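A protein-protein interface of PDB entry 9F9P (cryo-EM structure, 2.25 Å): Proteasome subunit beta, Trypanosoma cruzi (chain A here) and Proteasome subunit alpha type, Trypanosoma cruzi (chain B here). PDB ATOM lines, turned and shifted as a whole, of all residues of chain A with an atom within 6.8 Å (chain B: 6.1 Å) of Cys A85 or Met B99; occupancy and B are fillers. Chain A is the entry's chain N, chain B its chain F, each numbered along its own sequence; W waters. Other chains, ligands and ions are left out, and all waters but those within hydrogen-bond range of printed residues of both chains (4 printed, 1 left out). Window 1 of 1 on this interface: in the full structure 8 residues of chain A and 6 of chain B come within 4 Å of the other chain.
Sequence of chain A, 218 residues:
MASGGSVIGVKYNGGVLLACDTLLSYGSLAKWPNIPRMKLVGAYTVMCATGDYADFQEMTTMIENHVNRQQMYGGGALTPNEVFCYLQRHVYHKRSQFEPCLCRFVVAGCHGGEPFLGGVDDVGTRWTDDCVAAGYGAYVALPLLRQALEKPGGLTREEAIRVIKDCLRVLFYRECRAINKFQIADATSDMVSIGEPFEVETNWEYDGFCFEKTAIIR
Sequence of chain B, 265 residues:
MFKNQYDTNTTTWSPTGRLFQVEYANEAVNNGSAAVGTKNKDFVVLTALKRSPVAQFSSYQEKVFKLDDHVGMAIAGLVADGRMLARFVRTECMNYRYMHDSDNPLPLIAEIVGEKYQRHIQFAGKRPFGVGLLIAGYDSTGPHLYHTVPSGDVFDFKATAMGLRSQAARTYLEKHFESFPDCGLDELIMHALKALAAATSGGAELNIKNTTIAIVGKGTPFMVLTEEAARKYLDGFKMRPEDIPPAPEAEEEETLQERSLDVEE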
ATOM      1  N   PRO A  80     -24.287   9.219  -7.766  1.00  0.00           N
ATOM      2  CA  PRO A  80     -24.381   7.915  -7.122  1.00  0.00           C
ATOM      3  C   PRO A  80     -23.068   7.439  -6.547  1.00  0.00           C
ATOM      4  O   PRO A  80     -23.049   6.875  -5.471  1.00  0.00           O
ATOM      5  CB  PRO A  80     -24.828   6.951  -8.225  1.00  0.00           C
ATOM      6  CG  PRO A  80     -25.362   7.822  -9.356  1.00  0.00           C
ATOM      7  CD  PRO A  80     -24.756   9.198  -9.150  1.00  0.00           C
ATOM      8  N   ASN A  81     -21.990   7.721  -7.276  1.00  0.00           N
ATOM      9  CA  ASN A  81     -20.646   7.434  -6.794  1.00  0.00           C
ATOM     10  C   ASN A  81     -20.321   8.123  -5.474  1.00  0.00           C
ATOM     11  O   ASN A  81     -19.772   7.472  -4.590  1.00  0.00           O
ATOM     12  CB  ASN A  81     -19.598   7.732  -7.861  1.00  0.00           C
ATOM     13  CG  ASN A  81     -18.432   6.791  -7.684  1.00  0.00           C
ATOM     14  OD1 ASN A  81     -18.499   5.638  -8.114  1.00  0.00           O
ATOM     15  ND2 ASN A  81     -17.378   7.252  -7.004  1.00  0.00           N
ATOM     16  N   GLU A  82     -20.715   9.376  -5.287  1.00  0.00           N
ATOM     17  CA  GLU A  82     -20.456  10.121  -4.057  1.00  0.00           C
ATOM     18  C   GLU A  82     -21.328   9.669  -2.899  1.00  0.00           C
ATOM     19  O   GLU A  82     -20.838   9.503  -1.791  1.00  0.00           O
ATOM     20  CB  GLU A  82     -20.735  11.618  -4.266  1.00  0.00           C
ATOM     21  CG  GLU A  82     -19.865  12.274  -5.345  1.00  0.00           C
ATOM     22  CD  GLU A  82     -20.158  13.724  -5.743  1.00  0.00           C
ATOM     23  OE1 GLU A  82     -21.146  14.006  -6.496  1.00  0.00           O
ATOM     24  OE2 GLU A  82     -19.389  14.611  -5.289  1.00  0.00           O
ATOM     25  N   VAL A  83     -22.621   9.456  -3.169  1.00  0.00           N
ATOM     26  CA  VAL A  83     -23.542   8.883  -2.201  1.00  0.00           C
ATOM     27  C   VAL A  83     -23.039   7.541  -1.653  1.00  0.00           C
ATOM     28  O   VAL A  83     -23.183   7.261  -0.479  1.00  0.00           O
ATOM     29  CB  VAL A  83     -24.921   8.707  -2.846  1.00  0.00           C
ATOM     30  CG1 VAL A  83     -25.939   8.000  -1.956  1.00  0.00           C
ATOM     31  CG2 VAL A  83     -25.504  10.032  -3.264  1.00  0.00           C
ATOM     32  N   PHE A  84     -22.482   6.709  -2.514  1.00  0.00           N
ATOM     33  CA  PHE A  84     -22.004   5.391  -2.156  1.00  0.00           C
ATOM     34  C   PHE A  84     -20.808   5.430  -1.217  1.00  0.00           C
ATOM     35  O   PHE A  84     -20.728   4.684  -0.253  1.00  0.00           O
ATOM     36  CB  PHE A  84     -21.626   4.660  -3.439  1.00  0.00           C
ATOM     37  CG  PHE A  84     -21.220   3.215  -3.289  1.00  0.00           C
ATOM     38  CD1 PHE A  84     -22.160   2.248  -2.980  1.00  0.00           C
ATOM     39  CD2 PHE A  84     -19.909   2.820  -3.476  1.00  0.00           C
ATOM     40  CE1 PHE A  84     -21.804   0.919  -2.851  1.00  0.00           C
ATOM     41  CE2 PHE A  84     -19.562   1.478  -3.400  1.00  0.00           C
ATOM     42  CZ  PHE A  84     -20.505   0.531  -3.063  1.00  0.00           C
ATOM     43  N   CYS A  85     -19.837   6.276  -1.571  1.00  0.00           N
ATOM     44  CA  CYS A  85     -18.699   6.605  -0.728  1.00  0.00           C
ATOM     45  C   CYS A  85     -19.102   7.098   0.649  1.00  0.00           C
ATOM     46  O   CYS A  85     -18.600   6.605   1.619  1.00  0.00           O
ATOM     47  CB  CYS A  85     -17.786   7.619  -1.406  1.00  0.00           C
ATOM     48  SG  CYS A  85     -16.234   7.858  -0.471  1.00  0.00           S
ATOM     49  N   TYR A  86     -20.080   7.974   0.738  1.00  0.00           N
ATOM     50  CA  TYR A  86     -20.555   8.533   1.987  1.00  0.00           C
ATOM     51  C   TYR A  86     -21.219   7.478   2.863  1.00  0.00           C
ATOM     52  O   TYR A  86     -21.040   7.423   4.068  1.00  0.00           O
ATOM     53  CB  TYR A  86     -21.549   9.633   1.616  1.00  0.00           C
ATOM     54  CG  TYR A  86     -21.941  10.588   2.719  1.00  0.00           C
ATOM     55  CD1 TYR A  86     -21.099  11.626   3.078  1.00  0.00           C
ATOM     56  CD2 TYR A  86     -23.098  10.433   3.444  1.00  0.00           C
ATOM     57  CE1 TYR A  86     -21.418  12.507   4.080  1.00  0.00           C
ATOM     58  CE2 TYR A  86     -23.431  11.296   4.476  1.00  0.00           C
ATOM     59  CZ  TYR A  86     -22.594  12.352   4.773  1.00  0.00           C
ATOM     60  OH  TYR A  86     -22.854  13.267   5.754  1.00  0.00           O
ATOM     61  N   LEU A  87     -22.041   6.631   2.241  1.00  0.00           N
ATOM     62  CA  LEU A  87     -22.666   5.517   2.936  1.00  0.00           C
ATOM     63  C   LEU A  87     -21.613   4.613   3.565  1.00  0.00           C
ATOM     64  O   LEU A  87     -21.664   4.337   4.740  1.00  0.00           O
ATOM     65  CB  LEU A  87     -23.607   4.787   1.970  1.00  0.00           C
ATOM     66  CG  LEU A  87     -24.085   3.415   2.475  1.00  0.00           C
ATOM     67  CD1 LEU A  87     -25.114   3.570   3.564  1.00  0.00           C
ATOM     68  CD2 LEU A  87     -24.642   2.513   1.376  1.00  0.00           C
ATOM     69  N   GLN A  88     -20.612   4.232   2.799  1.00  0.00           N
ATOM     70  CA  GLN A  88     -19.564   3.334   3.256  1.00  0.00           C
ATOM     71  C   GLN A  88     -18.745   3.880   4.427  1.00  0.00           C
ATOM     72  O   GLN A  88     -18.395   3.119   5.299  1.00  0.00           O
ATOM     73  CB  GLN A  88     -18.637   2.928   2.111  1.00  0.00           C
ATOM     74  CG  GLN A  88     -17.649   1.825   2.515  1.00  0.00           C
ATOM     75  CD  GLN A  88     -16.323   2.265   3.108  1.00  0.00           C
ATOM     76  OE1 GLN A  88     -15.837   3.380   2.902  1.00  0.00           O
ATOM     77  NE2 GLN A  88     -15.685   1.359   3.830  1.00  0.00           N
ATOM     78  N   ARG A  89     -18.474   5.186   4.485  1.00  0.00           N
ATOM     79  CA  ARG A  89     -17.737   5.763   5.599  1.00  0.00           C
ATOM     80  C   ARG A  89     -18.564   5.791   6.876  1.00  0.00           C
ATOM     81  O   ARG A  89     -18.019   5.580   7.934  1.00  0.00           O
ATOM     82  CB  ARG A  89     -17.277   7.184   5.254  1.00  0.00           C
ATOM     83  CG  ARG A  89     -16.356   7.289   4.061  1.00  0.00           C
ATOM     84  CD  ARG A  89     -14.985   6.598   4.173  1.00  0.00           C
ATOM     85  NE  ARG A  89     -14.196   7.006   3.000  1.00  0.00           N
ATOM     86  CZ  ARG A  89     -13.172   6.358   2.449  1.00  0.00           C
ATOM     87  NH1 ARG A  89     -12.570   6.853   1.372  1.00  0.00           N
ATOM     88  NH2 ARG A  89     -12.793   5.188   2.916  1.00  0.00           N
ATOM     89  N   HIS A  90     -19.879   6.006   6.770  1.00  0.00           N
ATOM     90  CA  HIS A  90     -20.786   5.915   7.912  1.00  0.00           C
ATOM     91  C   HIS A  90     -20.877   4.503   8.497  1.00  0.00           C
ATOM     92  O   HIS A  90     -20.745   4.353   9.694  1.00  0.00           O
ATOM     93  CB  HIS A  90     -22.140   6.565   7.607  1.00  0.00           C
ATOM     94  CG  HIS A  90     -22.046   8.057   7.740  1.00  0.00           C
ATOM     95  ND1 HIS A  90     -22.130   8.679   8.975  1.00  0.00           N
ATOM     96  CD2 HIS A  90     -21.654   9.044   6.859  1.00  0.00           C
ATOM     97  CE1 HIS A  90     -21.919  10.001   8.824  1.00  0.00           C
ATOM     98  NE2 HIS A  90     -21.618  10.249   7.560  1.00  0.00           N
ATOM     99  N   PHE A 116     -24.549   2.902 -12.423  1.00  0.00           N
ATOM    100  CA  PHE A 116     -23.790   2.527 -11.247  1.00  0.00           C
ATOM    101  C   PHE A 116     -24.434   1.344 -10.521  1.00  0.00           C
ATOM    102  O   PHE A 116     -25.625   1.280 -10.398  1.00  0.00           O
ATOM    103  CB  PHE A 116     -23.667   3.792 -10.378  1.00  0.00           C
ATOM    104  CG  PHE A 116     -22.956   3.546  -9.091  1.00  0.00           C
ATOM    105  CD1 PHE A 116     -21.588   3.609  -9.044  1.00  0.00           C
ATOM    106  CD2 PHE A 116     -23.661   3.073  -7.993  1.00  0.00           C
ATOM    107  CE1 PHE A 116     -20.911   3.305  -7.889  1.00  0.00           C
ATOM    108  CE2 PHE A 116     -22.978   2.690  -6.844  1.00  0.00           C
ATOM    109  CZ  PHE A 116     -21.604   2.860  -6.777  1.00  0.00           C
ATOM    110  N   ARG A 126     -16.762  -2.945   0.507  1.00  0.00           N
ATOM    111  CA  ARG A 126     -17.470  -2.364  -0.609  1.00  0.00           C
ATOM    112  C   ARG A 126     -16.968  -2.872  -1.948  1.00  0.00           C
ATOM    113  O   ARG A 126     -15.803  -3.101  -2.093  1.00  0.00           O
ATOM    114  CB  ARG A 126     -17.411  -0.834  -0.599  1.00  0.00           C
ATOM    115  CG  ARG A 126     -16.022  -0.228  -0.502  1.00  0.00           C
ATOM    116  CD  ARG A 126     -16.020   1.236  -0.907  1.00  0.00           C
ATOM    117  NE  ARG A 126     -15.919   1.404  -2.337  1.00  0.00           N
ATOM    118  CZ  ARG A 126     -16.231   2.530  -2.971  1.00  0.00           C
ATOM    119  NH1 ARG A 126     -16.496   3.634  -2.291  1.00  0.00           N
ATOM    120  NH2 ARG A 126     -16.240   2.568  -4.295  1.00  0.00           N
ATOM    121  N   MET B  94      -9.560  18.117   2.747  1.00  0.00           N
ATOM    122  CA  MET B  94      -9.210  16.736   2.965  1.00  0.00           C
ATOM    123  C   MET B  94     -10.413  15.948   3.496  1.00  0.00           C
ATOM    124  O   MET B  94     -10.686  14.860   3.001  1.00  0.00           O
ATOM    125  CB  MET B  94      -8.043  16.584   3.938  1.00  0.00           C
ATOM    126  CG  MET B  94      -6.689  16.820   3.292  1.00  0.00           C
ATOM    127  SD  MET B  94      -5.325  16.706   4.496  1.00  0.00           S
ATOM    128  CE  MET B  94      -4.136  17.793   3.732  1.00  0.00           C
ATOM    129  N   ASN B  95     -11.128  16.464   4.484  1.00  0.00           N
ATOM    130  CA  ASN B  95     -12.330  15.788   4.916  1.00  0.00           C
ATOM    131  C   ASN B  95     -13.374  15.616   3.801  1.00  0.00           C
ATOM    132  O   ASN B  95     -13.971  14.566   3.686  1.00  0.00           O
ATOM    133  CB  ASN B  95     -13.056  16.513   6.035  1.00  0.00           C
ATOM    134  CG  ASN B  95     -12.263  16.596   7.304  1.00  0.00           C
ATOM    135  OD1 ASN B  95     -11.333  15.834   7.529  1.00  0.00           O
ATOM    136  ND2 ASN B  95     -12.601  17.571   8.142  1.00  0.00           N
ATOM    137  N   TYR B  96     -13.619  16.629   2.996  1.00  0.00           N
ATOM    138  CA  TYR B  96     -14.590  16.484   1.949  1.00  0.00           C
ATOM    139  C   TYR B  96     -14.237  15.323   1.009  1.00  0.00           C
ATOM    140  O   TYR B  96     -15.110  14.534   0.649  1.00  0.00           O
ATOM    141  CB  TYR B  96     -14.773  17.770   1.146  1.00  0.00           C
ATOM    142  CG  TYR B  96     -15.984  17.757   0.238  1.00  0.00           C
ATOM    143  CD1 TYR B  96     -17.216  18.180   0.699  1.00  0.00           C
ATOM    144  CD2 TYR B  96     -15.908  17.242  -1.048  1.00  0.00           C
ATOM    145  CE1 TYR B  96     -18.359  18.099  -0.094  1.00  0.00           C
ATOM    146  CE2 TYR B  96     -17.033  17.183  -1.875  1.00  0.00           C
ATOM    147  CZ  TYR B  96     -18.272  17.592  -1.382  1.00  0.00           C
ATOM    148  OH  TYR B  96     -19.405  17.525  -2.175  1.00  0.00           O
ATOM    149  N   ARG B  97     -12.979  15.212   0.620  1.00  0.00           N
ATOM    150  CA  ARG B  97     -12.569  14.170  -0.304  1.00  0.00           C
ATOM    151  C   ARG B  97     -12.634  12.780   0.362  1.00  0.00           C
ATOM    152  O   ARG B  97     -13.044  11.811  -0.247  1.00  0.00           O
ATOM    153  CB  ARG B  97     -11.179  14.480  -0.866  1.00  0.00           C
ATOM    154  CG  ARG B  97     -10.897  13.692  -2.136  1.00  0.00           C
ATOM    155  CD  ARG B  97      -9.514  13.830  -2.751  1.00  0.00           C
ATOM    156  NE  ARG B  97      -9.252  15.199  -3.125  1.00  0.00           N
ATOM    157  CZ  ARG B  97      -9.674  15.720  -4.260  1.00  0.00           C
ATOM    158  NH1 ARG B  97     -10.309  14.935  -5.135  1.00  0.00           N
ATOM    159  NH2 ARG B  97      -9.488  17.010  -4.497  1.00  0.00           N
ATOM    160  N   TYR B  98     -12.292  12.688   1.631  1.00  0.00           N
ATOM    161  CA  TYR B  98     -12.446  11.442   2.347  1.00  0.00           C
ATOM    162  C   TYR B  98     -13.900  10.954   2.258  1.00  0.00           C
ATOM    163  O   TYR B  98     -14.156   9.802   1.898  1.00  0.00           O
ATOM    164  CB  TYR B  98     -11.977  11.602   3.783  1.00  0.00           C
ATOM    165  CG  TYR B  98     -12.197  10.407   4.655  1.00  0.00           C
ATOM    166  CD1 TYR B  98     -11.405   9.279   4.531  1.00  0.00           C
ATOM    167  CD2 TYR B  98     -13.216  10.391   5.621  1.00  0.00           C
ATOM    168  CE1 TYR B  98     -11.603   8.177   5.362  1.00  0.00           C
ATOM    169  CE2 TYR B  98     -13.415   9.301   6.477  1.00  0.00           C
ATOM    170  CZ  TYR B  98     -12.584   8.196   6.351  1.00  0.00           C
ATOM    171  OH  TYR B  98     -12.778   7.075   7.099  1.00  0.00           O
ATOM    172  N   MET B  99     -14.858  11.827   2.532  1.00  0.00           N
ATOM    173  CA  MET B  99     -16.247  11.418   2.609  1.00  0.00           C
ATOM    174  C   MET B  99     -16.883  11.280   1.240  1.00  0.00           C
ATOM    175  O   MET B  99     -17.795  10.505   1.146  1.00  0.00           O
ATOM    176  CB  MET B  99     -17.069  12.411   3.417  1.00  0.00           C
ATOM    177  CG  MET B  99     -16.656  12.519   4.864  1.00  0.00           C
ATOM    178  SD  MET B  99     -16.938  11.009   5.870  1.00  0.00           S
ATOM    179  CE  MET B  99     -18.722  10.864   5.846  1.00  0.00           C
ATOM    180  N   HIS B 100     -16.436  11.942   0.178  1.00  0.00           N
ATOM    181  CA  HIS B 100     -17.165  11.912  -1.078  1.00  0.00           C
ATOM    182  C   HIS B 100     -16.378  11.398  -2.271  1.00  0.00           C
ATOM    183  O   HIS B 100     -16.937  11.263  -3.356  1.00  0.00           O
ATOM    184  CB  HIS B 100     -17.692  13.303  -1.470  1.00  0.00           C
ATOM    185  CG  HIS B 100     -18.522  13.970  -0.416  1.00  0.00           C
ATOM    186  ND1 HIS B 100     -17.957  14.642   0.627  1.00  0.00           N
ATOM    187  CD2 HIS B 100     -19.837  14.070  -0.289  1.00  0.00           C
ATOM    188  CE1 HIS B 100     -18.906  15.107   1.400  1.00  0.00           C
ATOM    189  NE2 HIS B 100     -20.122  14.787   0.873  1.00  0.00           N
ATOM    190  N   ASP B 101     -15.077  11.232  -2.141  1.00  0.00           N
ATOM    191  CA  ASP B 101     -14.229  10.917  -3.286  1.00  0.00           C
ATOM    192  C   ASP B 101     -14.327  11.930  -4.432  1.00  0.00           C
ATOM    193  O   ASP B 101     -14.233  11.542  -5.587  1.00  0.00           O
ATOM    194  CB  ASP B 101     -14.549   9.497  -3.777  1.00  0.00           C
ATOM    195  CG  ASP B 101     -13.523   8.918  -4.753  1.00  0.00           C
ATOM    196  OD1 ASP B 101     -12.287   9.064  -4.474  1.00  0.00           O
ATOM    197  OD2 ASP B 101     -13.957   8.316  -5.798  1.00  0.00           O
HETATM  198  O   HOH W   1     -19.106  17.151  -4.769  1.00  0.00           O
HETATM  199  O   HOH W   2     -13.204   4.125   5.424  1.00  0.00           O
HETATM  200  O   HOH W   3     -12.456   9.005  -0.736  1.00  0.00           O
HETATM  201  O   HOH W   4     -17.341   9.843  -5.938  1.00  0.00           O
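Printed residues of chain B within 4 Å of Asn A81: Asp B101.
Of the printed residues of chain B, Glu A82 touches His B100 (3.7 Å).
Of the printed residues of chain B, Cys A85 touches Tyr B98, Met B99, His B100 and Asp B101.
Printed residues of chain B within 4 Å of His A90: Met B99 (3.4 Å).
Of chain A, only Cys A85 (3.5 Å), Tyr A86 (3.4 Å), Arg A89 (3.9 Å) and His A90 (3.4 Å) come within 4 Å of Met B99.
The nearest residue of chain A that does not touch Met B99 is Glu A82 (4.3 Å).
Water W1 lies within hydrogen-bond range of the side-chain carboxylate of Glu A82 and the side-chain hydroxyl of Tyr B96.
Water W2 lies within hydrogen-bond range of NH2 of Arg A89 (2.8 Å) and OH of Tyr B98 (3.4 Å).
Water W4 lies within hydrogen-bond range of the side-chain amide nitrogen of Asn A81, the backbone carbonyl oxygen of His B100 and the backbone NH of Glu A82.
Water W3 lies within hydrogen-bond range of the backbone carbonyl oxygen (O) of Arg B97, the guanidinium group (NH1) of Arg A89 and the backbone carbonyl oxygen (O) of Tyr B98.
The backbone carbonyl oxygen (O) of Tyr B98 is in hydrogen-bond range of the side-chain sulfur (SG) of Cys A85.
The side-chain sulfur (SG) of Cys A85 lies within hydrogen-bond range of the backbone carbonyl oxygen (O) of Met B99 (3.5 Å).
O of Met B99 is in hydrogen-bond range of N of Tyr A86 (3.4 Å).
The backbone carbonyl oxygen of Tyr B98 is in hydrogen-bond range of the guanidinium group of Arg A89.
The backbone carbonyl oxygen (O) of Tyr B96 lies within hydrogen-bond range of a ring nitrogen (ND1) of His B100 (2.8 Å).
Among the printed residues, pairs that only touch across the chains: His A90 with Met B99 (3.4 Å), Glu A82 with His B100 (3.7 Å), Asn A81 with Asp B101 (3.8 Å), Arg A89 with Met B99 (3.9 Å), Cys A85 with Asp B101 (3.9 Å), Cys A85 with His B100 (3.97 Å) and Tyr A86 with His B100 (3.98 Å).
Of the 8 printed residues of chain B, 4 touch a printed residue of chain A.
Hydrophobic or aromatic side chains of chain B within 4 Å of the printed part of chain A: Tyr B98, Met B99 and His B100.
Of the 13 printed residues of chain A, 6 touch a printed residue of chain B.
Hydrophobic or aromatic side chains of chain A within 4 Å of the printed part of chain B: Tyr A86 and His A90.
Along chain A the printed residues that touch a printed residue of chain B span positions 81 to 90.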
